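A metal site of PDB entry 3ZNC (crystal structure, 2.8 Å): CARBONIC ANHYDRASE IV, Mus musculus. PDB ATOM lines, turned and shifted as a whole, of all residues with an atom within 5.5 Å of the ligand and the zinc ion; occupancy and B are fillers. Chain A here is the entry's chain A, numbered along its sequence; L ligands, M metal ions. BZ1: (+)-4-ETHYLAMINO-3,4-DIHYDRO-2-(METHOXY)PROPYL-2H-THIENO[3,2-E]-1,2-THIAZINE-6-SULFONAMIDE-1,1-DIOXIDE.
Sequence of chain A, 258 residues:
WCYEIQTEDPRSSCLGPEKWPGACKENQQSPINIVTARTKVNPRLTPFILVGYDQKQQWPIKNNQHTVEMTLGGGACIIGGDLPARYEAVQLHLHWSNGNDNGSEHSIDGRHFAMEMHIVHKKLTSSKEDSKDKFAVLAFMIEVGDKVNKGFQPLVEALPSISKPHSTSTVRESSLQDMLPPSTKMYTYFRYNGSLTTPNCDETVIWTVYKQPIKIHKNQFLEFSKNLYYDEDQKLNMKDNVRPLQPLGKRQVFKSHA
The zinc ion is bound by N2 of the ligand (1.9 Å), NE2 of His 93 (2.0 Å), NE2 of His 95 (2.1 Å) and ND1 of His 118 (2.3 Å).
Slightly farther from the zinc ion lies an oxygen (O4) of the ligand (2.8 Å).
The backbone NH (N) of Thr 197 lies within hydrogen-bond range of an oxygen (O3) of the ligand, at 2.8 Å.
The side-chain hydroxyl (OG1) of Thr 197 sits at hydrogen-bond distance from an oxygen (O3) of the ligand (3.2 Å).
The side-chain amide nitrogen (NE2) of Gln 91 is in hydrogen-bond range of an oxygen (O5) of the ligand, 2.8 Å away.
A nitrogen (N1) of the ligand sits at hydrogen-bond distance from the side-chain hydroxyl (OG1) of Thr 198 (3.1 Å).
Residues that only touch the ligand: Val 120, Phe 135, Leu 196 and Trp 207.
Thr 197 touches the zinc ion (OG1 to ZN, 3.8 Å).
Four residues have an atom within 4 Å of the zinc ion: His 93, His 95, His 118 and Thr 197.
Along chain A the residues within 4 Å of the zinc ion span positions 93 to 197.
The nearest printed residue that does not touch the zinc ion is Glu 105 (4.1 Å).
OE1 of Gln 91 lies within hydrogen-bond range of ND1 of His 93.
ND1 of His 95 sits close to OE2 of Glu 105, 3.5 Å away.
OE1 of Glu 105 lies within hydrogen-bond range of OG1 of Thr 197 (2.9 Å).
The backbone NH (N) of Val 120 lies within hydrogen-bond range of the backbone carbonyl oxygen (O) of Gln 91, 3.0 Å away.
The side-chain amide nitrogen (NE2) of Gln 91 is in hydrogen-bond range of the side-chain carboxylate (OE2) of Glu 69 (3.0 Å).
The backbone carbonyl oxygen of Val 120 sits at hydrogen-bond distance from the backbone NH of Val 90, 2.9 Å away.
The indole nitrogen of Trp 207 is in hydrogen-bond range of the backbone carbonyl oxygen of Ser 195 (3.1 Å).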
ATOM      1  N   TRP A   1       1.583  -6.298  24.086  1.00  0.00           N
ATOM      2  CA  TRP A   1       1.296  -6.219  22.619  1.00  0.00           C
ATOM      3  C   TRP A   1       2.521  -5.618  21.943  1.00  0.00           C
ATOM      4  O   TRP A   1       3.327  -4.946  22.598  1.00  0.00           O
ATOM      5  CB  TRP A   1       0.016  -5.330  22.339  1.00  0.00           C
ATOM      6  CG  TRP A   1       0.173  -3.851  22.626  1.00  0.00           C
ATOM      7  CD1 TRP A   1      -0.224  -3.183  23.751  1.00  0.00           C
ATOM      8  CD2 TRP A   1       0.727  -2.854  21.744  1.00  0.00           C
ATOM      9  NE1 TRP A   1       0.040  -1.831  23.626  1.00  0.00           N
ATOM     10  CE2 TRP A   1       0.618  -1.606  22.409  1.00  0.00           C
ATOM     11  CE3 TRP A   1       1.289  -2.897  20.465  1.00  0.00           C
ATOM     12  CZ2 TRP A   1       1.070  -0.421  21.831  1.00  0.00           C
ATOM     13  CZ3 TRP A   1       1.740  -1.713  19.887  1.00  0.00           C
ATOM     14  CH2 TRP A   1       1.622  -0.486  20.573  1.00  0.00           C
ATOM     15  N   ASN A  64       8.531   5.656  24.943  1.00  0.00           N
ATOM     16  CA  ASN A  64       7.498   4.896  25.645  1.00  0.00           C
ATOM     17  C   ASN A  64       7.469   3.418  25.301  1.00  0.00           C
ATOM     18  O   ASN A  64       6.528   2.717  25.670  1.00  0.00           O
ATOM     19  CB  ASN A  64       6.073   5.539  25.423  1.00  0.00           C
ATOM     20  CG  ASN A  64       5.627   5.504  23.974  1.00  0.00           C
ATOM     21  OD1 ASN A  64       6.198   4.798  23.142  1.00  0.00           O
ATOM     22  ND2 ASN A  64       4.581   6.267  23.667  1.00  0.00           N
ATOM     23  N   HIS A  66       7.257   2.273  22.296  1.00  0.00           N
ATOM     24  CA  HIS A  66       6.567   2.096  21.020  1.00  0.00           C
ATOM     25  C   HIS A  66       6.885   3.244  20.064  1.00  0.00           C
ATOM     26  O   HIS A  66       6.731   3.106  18.845  1.00  0.00           O
ATOM     27  CB  HIS A  66       5.023   1.994  21.223  1.00  0.00           C
ATOM     28  CG  HIS A  66       4.611   0.920  22.195  1.00  0.00           C
ATOM     29  ND1 HIS A  66       4.835  -0.421  21.965  1.00  0.00           N
ATOM     30  CD2 HIS A  66       4.003   0.990  23.404  1.00  0.00           C
ATOM     31  CE1 HIS A  66       4.377  -1.129  22.983  1.00  0.00           C
ATOM     32  NE2 HIS A  66       3.873  -0.291  23.871  1.00  0.00           N
ATOM     33  N   THR A  67       7.347   4.359  20.607  1.00  0.00           N
ATOM     34  CA  THR A  67       7.664   5.533  19.800  1.00  0.00           C
ATOM     35  C   THR A  67       8.309   6.583  20.694  1.00  0.00           C
ATOM     36  O   THR A  67       8.548   6.347  21.886  1.00  0.00           O
ATOM     37  CB  THR A  67       6.384   6.081  19.141  1.00  0.00           C
ATOM     38  OG1 THR A  67       6.689   7.210  18.319  1.00  0.00           O
ATOM     39  CG2 THR A  67       5.361   6.483  20.203  1.00  0.00           C
ATOM     40  N   GLU A  69       7.725   9.830  22.439  1.00  0.00           N
ATOM     41  CA  GLU A  69       6.621  10.659  22.900  1.00  0.00           C
ATOM     42  C   GLU A  69       7.106  12.025  23.392  1.00  0.00           C
ATOM     43  O   GLU A  69       8.073  12.122  24.132  1.00  0.00           O
ATOM     44  CB  GLU A  69       5.852   9.898  24.039  1.00  0.00           C
ATOM     45  CG  GLU A  69       4.514  10.501  24.426  1.00  0.00           C
ATOM     46  CD  GLU A  69       3.815   9.713  25.523  1.00  0.00           C
ATOM     47  OE1 GLU A  69       4.208   8.554  25.795  1.00  0.00           O
ATOM     48  OE2 GLU A  69       2.855  10.252  26.134  1.00  0.00           O
ATOM     49  N   VAL A  90      -2.043  17.331  23.533  1.00  0.00           N
ATOM     50  CA  VAL A  90      -1.628  16.480  24.649  1.00  0.00           C
ATOM     51  C   VAL A  90      -0.223  15.900  24.448  1.00  0.00           C
ATOM     52  O   VAL A  90       0.651  16.074  25.289  1.00  0.00           O
ATOM     53  CB  VAL A  90      -2.661  15.350  24.915  1.00  0.00           C
ATOM     54  CG1 VAL A  90      -1.991  14.118  25.526  1.00  0.00           C
ATOM     55  CG2 VAL A  90      -3.753  15.846  25.845  1.00  0.00           C
ATOM     56  N   GLN A  91       0.003  15.231  23.310  1.00  0.00           N
ATOM     57  CA  GLN A  91       1.292  14.617  23.010  1.00  0.00           C
ATOM     58  C   GLN A  91       1.584  14.645  21.513  1.00  0.00           C
ATOM     59  O   GLN A  91       0.721  14.952  20.701  1.00  0.00           O
ATOM     60  CB  GLN A  91       1.309  13.136  23.491  1.00  0.00           C
ATOM     61  CG  GLN A  91       0.549  12.204  22.575  1.00  0.00           C
ATOM     62  CD  GLN A  91       0.920  10.755  22.777  1.00  0.00           C
ATOM     63  OE1 GLN A  91       1.356  10.077  21.850  1.00  0.00           O
ATOM     64  NE2 GLN A  91       0.783  10.282  24.000  1.00  0.00           N
ATOM     65  N   HIS A  93       4.047  12.223  18.617  1.00  0.00           N
ATOM     66  CA  HIS A  93       4.932  11.093  18.384  1.00  0.00           C
ATOM     67  C   HIS A  93       5.041  10.832  16.891  1.00  0.00           C
ATOM     68  O   HIS A  93       4.416  11.536  16.094  1.00  0.00           O
ATOM     69  CB  HIS A  93       4.431   9.815  19.150  1.00  0.00           C
ATOM     70  CG  HIS A  93       3.105   9.299  18.680  1.00  0.00           C
ATOM     71  ND1 HIS A  93       1.921   9.510  19.341  1.00  0.00           N
ATOM     72  CD2 HIS A  93       2.795   8.552  17.601  1.00  0.00           C
ATOM     73  CE1 HIS A  93       0.948   8.893  18.658  1.00  0.00           C
ATOM     74  NE2 HIS A  93       1.430   8.295  17.585  1.00  0.00           N
ATOM     75  N   HIS A  95       5.914   7.625  13.577  1.00  0.00           N
ATOM     76  CA  HIS A  95       5.949   6.223  13.112  1.00  0.00           C
ATOM     77  C   HIS A  95       6.899   6.178  11.908  1.00  0.00           C
ATOM     78  O   HIS A  95       6.756   6.964  10.974  1.00  0.00           O
ATOM     79  CB  HIS A  95       4.527   5.724  12.659  1.00  0.00           C
ATOM     80  CG  HIS A  95       3.504   5.812  13.740  1.00  0.00           C
ATOM     81  ND1 HIS A  95       3.115   4.742  14.522  1.00  0.00           N
ATOM     82  CD2 HIS A  95       2.778   6.870  14.178  1.00  0.00           C
ATOM     83  CE1 HIS A  95       2.200   5.182  15.397  1.00  0.00           C
ATOM     84  NE2 HIS A  95       1.960   6.465  15.227  1.00  0.00           N
ATOM     85  N   GLU A 105       1.992   5.269   8.263  1.00  0.00           N
ATOM     86  CA  GLU A 105       0.879   4.360   8.437  1.00  0.00           C
ATOM     87  C   GLU A 105      -0.149   4.572   7.329  1.00  0.00           C
ATOM     88  O   GLU A 105      -0.484   3.639   6.599  1.00  0.00           O
ATOM     89  CB  GLU A 105       0.240   4.548   9.854  1.00  0.00           C
ATOM     90  CG  GLU A 105       1.207   4.186  10.972  1.00  0.00           C
ATOM     91  CD  GLU A 105       0.548   4.061  12.327  1.00  0.00           C
ATOM     92  OE1 GLU A 105       0.005   5.060  12.831  1.00  0.00           O
ATOM     93  OE2 GLU A 105       0.595   2.950  12.898  1.00  0.00           O
ATOM     94  N   HIS A 118       2.213  12.392  14.444  1.00  0.00           N
ATOM     95  CA  HIS A 118       0.896  12.461  15.028  1.00  0.00           C
ATOM     96  C   HIS A 118       0.790  13.370  16.240  1.00  0.00           C
ATOM     97  O   HIS A 118       1.348  13.080  17.294  1.00  0.00           O
ATOM     98  CB  HIS A 118       0.381  11.025  15.395  1.00  0.00           C
ATOM     99  CG  HIS A 118       0.058  10.187  14.202  1.00  0.00           C
ATOM    100  ND1 HIS A 118       0.143   8.814  14.234  1.00  0.00           N
ATOM    101  CD2 HIS A 118      -0.382  10.574  12.976  1.00  0.00           C
ATOM    102  CE1 HIS A 118      -0.251   8.402  13.047  1.00  0.00           C
ATOM    103  NE2 HIS A 118      -0.585   9.431  12.250  1.00  0.00           N
ATOM    104  N   VAL A 120      -1.608  14.536  18.864  1.00  0.00           N
ATOM    105  CA  VAL A 120      -2.870  14.164  19.496  1.00  0.00           C
ATOM    106  C   VAL A 120      -3.526  15.272  20.312  1.00  0.00           C
ATOM    107  O   VAL A 120      -2.857  15.944  21.093  1.00  0.00           O
ATOM    108  CB  VAL A 120      -2.682  12.926  20.400  1.00  0.00           C
ATOM    109  CG1 VAL A 120      -4.029  12.372  20.847  1.00  0.00           C
ATOM    110  CG2 VAL A 120      -1.890  11.861  19.677  1.00  0.00           C
ATOM    111  N   LYS A 122      -6.943  16.076  22.857  1.00  0.00           N
ATOM    112  CA  LYS A 122      -8.073  15.533  23.614  1.00  0.00           C
ATOM    113  C   LYS A 122      -9.226  16.546  23.575  1.00  0.00           C
ATOM    114  O   LYS A 122      -8.996  17.751  23.655  1.00  0.00           O
ATOM    115  CB  LYS A 122      -7.651  15.266  25.107  1.00  0.00           C
ATOM    116  CG  LYS A 122      -8.799  14.912  26.044  1.00  0.00           C
ATOM    117  CD  LYS A 122      -8.414  15.147  27.518  1.00  0.00           C
ATOM    118  CE  LYS A 122      -7.377  14.139  28.020  1.00  0.00           C
ATOM    119  NZ  LYS A 122      -7.914  12.742  28.106  1.00  0.00           N
ATOM    120  N   PHE A 135     -10.901  12.475  20.307  1.00  0.00           N
ATOM    121  CA  PHE A 135      -9.519  12.714  19.933  1.00  0.00           C
ATOM    122  C   PHE A 135      -9.482  13.325  18.539  1.00  0.00           C
ATOM    123  O   PHE A 135     -10.203  12.899  17.648  1.00  0.00           O
ATOM    124  CB  PHE A 135      -8.714  11.381  19.936  1.00  0.00           C
ATOM    125  CG  PHE A 135      -8.272  10.948  21.284  1.00  0.00           C
ATOM    126  CD1 PHE A 135      -7.353  11.702  22.001  1.00  0.00           C
ATOM    127  CD2 PHE A 135      -8.755   9.780  21.850  1.00  0.00           C
ATOM    128  CE1 PHE A 135      -6.915  11.295  23.263  1.00  0.00           C
ATOM    129  CE2 PHE A 135      -8.335   9.363  23.103  1.00  0.00           C
ATOM    130  CZ  PHE A 135      -7.404  10.118  23.807  1.00  0.00           C
ATOM    131  N   VAL A 137      -6.668  13.922  15.915  1.00  0.00           N
ATOM    132  CA  VAL A 137      -5.273  13.651  15.608  1.00  0.00           C
ATOM    133  C   VAL A 137      -4.905  14.258  14.261  1.00  0.00           C
ATOM    134  O   VAL A 137      -5.564  13.993  13.247  1.00  0.00           O
ATOM    135  CB  VAL A 137      -4.986  12.118  15.581  1.00  0.00           C
ATOM    136  CG1 VAL A 137      -3.522  11.861  15.189  1.00  0.00           C
ATOM    137  CG2 VAL A 137      -5.282  11.501  16.944  1.00  0.00           C
ATOM    138  N   SER A 195      -9.906   5.410  14.354  1.00  0.00           N
ATOM    139  CA  SER A 195      -9.477   5.003  15.687  1.00  0.00           C
ATOM    140  C   SER A 195      -7.985   5.171  15.947  1.00  0.00           C
ATOM    141  O   SER A 195      -7.223   5.559  15.048  1.00  0.00           O
ATOM    142  CB  SER A 195      -9.828   3.485  15.890  1.00  0.00           C
ATOM    143  OG  SER A 195      -9.194   2.696  14.881  1.00  0.00           O
ATOM    144  N   LEU A 196      -7.573   4.894  17.182  1.00  0.00           N
ATOM    145  CA  LEU A 196      -6.157   4.926  17.549  1.00  0.00           C
ATOM    146  C   LEU A 196      -5.529   3.814  16.715  1.00  0.00           C
ATOM    147  O   LEU A 196      -6.161   2.772  16.493  1.00  0.00           O
ATOM    148  CB  LEU A 196      -5.978   4.556  19.072  1.00  0.00           C
ATOM    149  CG  LEU A 196      -6.105   5.583  20.244  1.00  0.00           C
ATOM    150  CD1 LEU A 196      -7.298   6.480  20.081  1.00  0.00           C
ATOM    151  CD2 LEU A 196      -6.201   4.819  21.548  1.00  0.00           C
ATOM    152  N   THR A 197      -4.293   3.996  16.275  1.00  0.00           N
ATOM    153  CA  THR A 197      -3.623   2.997  15.466  1.00  0.00           C
ATOM    154  C   THR A 197      -2.862   1.948  16.292  1.00  0.00           C
ATOM    155  O   THR A 197      -2.154   1.106  15.756  1.00  0.00           O
ATOM    156  CB  THR A 197      -2.700   3.653  14.433  1.00  0.00           C
ATOM    157  OG1 THR A 197      -1.732   4.483  15.083  1.00  0.00           O
ATOM    158  CG2 THR A 197      -3.516   4.490  13.461  1.00  0.00           C
ATOM    159  N   THR A 198      -3.007   2.021  17.620  1.00  0.00           N
ATOM    160  CA  THR A 198      -2.376   1.093  18.550  1.00  0.00           C
ATOM    161  C   THR A 198      -3.481   0.639  19.501  1.00  0.00           C
ATOM    162  O   THR A 198      -4.525   1.285  19.581  1.00  0.00           O
ATOM    163  CB  THR A 198      -1.245   1.772  19.371  1.00  0.00           C
ATOM    164  OG1 THR A 198      -1.779   2.852  20.131  1.00  0.00           O
ATOM    165  CG2 THR A 198      -0.155   2.298  18.460  1.00  0.00           C
ATOM    166  N   PRO A 199      -3.278  -0.482  20.227  1.00  0.00           N
ATOM    167  CA  PRO A 199      -4.306  -0.955  21.159  1.00  0.00           C
ATOM    168  C   PRO A 199      -4.628   0.113  22.208  1.00  0.00           C
ATOM    169  O   PRO A 199      -3.765   0.926  22.554  1.00  0.00           O
ATOM    170  CB  PRO A 199      -3.627  -2.220  21.808  1.00  0.00           C
ATOM    171  CG  PRO A 199      -2.752  -2.701  20.716  1.00  0.00           C
ATOM    172  CD  PRO A 199      -2.138  -1.414  20.191  1.00  0.00           C
ATOM    173  N   TRP A 207      -9.773  12.040  12.364  1.00  0.00           N
ATOM    174  CA  TRP A 207      -8.486  12.206  11.674  1.00  0.00           C
ATOM    175  C   TRP A 207      -8.415  13.303  10.633  1.00  0.00           C
ATOM    176  O   TRP A 207      -9.345  13.488   9.843  1.00  0.00           O
ATOM    177  CB  TRP A 207      -8.037  10.867  10.987  1.00  0.00           C
ATOM    178  CG  TRP A 207      -7.552   9.813  11.923  1.00  0.00           C
ATOM    179  CD1 TRP A 207      -8.313   8.858  12.531  1.00  0.00           C
ATOM    180  CD2 TRP A 207      -6.202   9.603  12.364  1.00  0.00           C
ATOM    181  NE1 TRP A 207      -7.513   8.064  13.322  1.00  0.00           N
ATOM    182  CE2 TRP A 207      -6.221   8.500  13.234  1.00  0.00           C
ATOM    183  CE3 TRP A 207      -4.992  10.251  12.106  1.00  0.00           C
ATOM    184  CZ2 TRP A 207      -5.056   8.013  13.843  1.00  0.00           C
ATOM    185  CZ3 TRP A 207      -3.836   9.769  12.706  1.00  0.00           C
ATOM    186  CH2 TRP A 207      -3.875   8.664  13.574  1.00  0.00           C
HETATM  187  C3  BZ1 L   1      -4.884   6.149  25.664  1.00  0.00           C
HETATM  188  C9  BZ1 L   1      -2.117   6.227  21.277  1.00  0.00           C
HETATM  189  C10 BZ1 L   1      -2.628   7.678  21.493  1.00  0.00           C
HETATM  190  C11 BZ1 L   1      -1.868   5.270  22.461  1.00  0.00           C
HETATM  191  C12 BZ1 L   1      -1.836   6.038  23.799  1.00  0.00           C
HETATM  192  S1  BZ1 L   1      -2.193   7.245  17.485  1.00  0.00           S
HETATM  193  C4  BZ1 L   1      -6.243   6.840  25.777  1.00  0.00           C
HETATM  194  C5  BZ1 L   1       1.317   5.435  21.270  1.00  0.00           C
HETATM  195  C6  BZ1 L   1       0.717   5.219  22.662  1.00  0.00           C
HETATM  196  S2  BZ1 L   1      -2.905   8.541  19.958  1.00  0.00           S
HETATM  197  N2  BZ1 L   1      -0.905   6.373  16.897  1.00  0.00           N
HETATM  198  O3  BZ1 L   1      -3.404   6.655  16.638  1.00  0.00           O
HETATM  199  O4  BZ1 L   1      -1.841   8.755  17.204  1.00  0.00           O
HETATM  200  C7  BZ1 L   1      -2.259   7.070  19.224  1.00  0.00           C
HETATM  201  C8  BZ1 L   1      -1.926   6.018  19.971  1.00  0.00           C
HETATM  202  S3  BZ1 L   1      -2.957   8.286  23.153  1.00  0.00           S
HETATM  203  O2  BZ1 L   1      -4.355   9.026  23.189  1.00  0.00           O
HETATM  204  O5  BZ1 L   1      -1.826   9.270  23.699  1.00  0.00           O
HETATM  205  N3  BZ1 L   1      -3.021   6.888  24.143  1.00  0.00           N
HETATM  206  N1  BZ1 L   1      -0.571   4.482  22.478  1.00  0.00           N
HETATM  207  C2  BZ1 L   1      -4.356   6.247  24.244  1.00  0.00           C
HETATM  208  O1  BZ1 L   1      -6.116   8.025  26.585  1.00  0.00           O
HETATM  209  C1  BZ1 L   1      -5.824   7.952  28.003  1.00  0.00           C
HETATM  210 ZN    ZN M   1       0.388   7.506  16.049  1.00  0.00          ZN
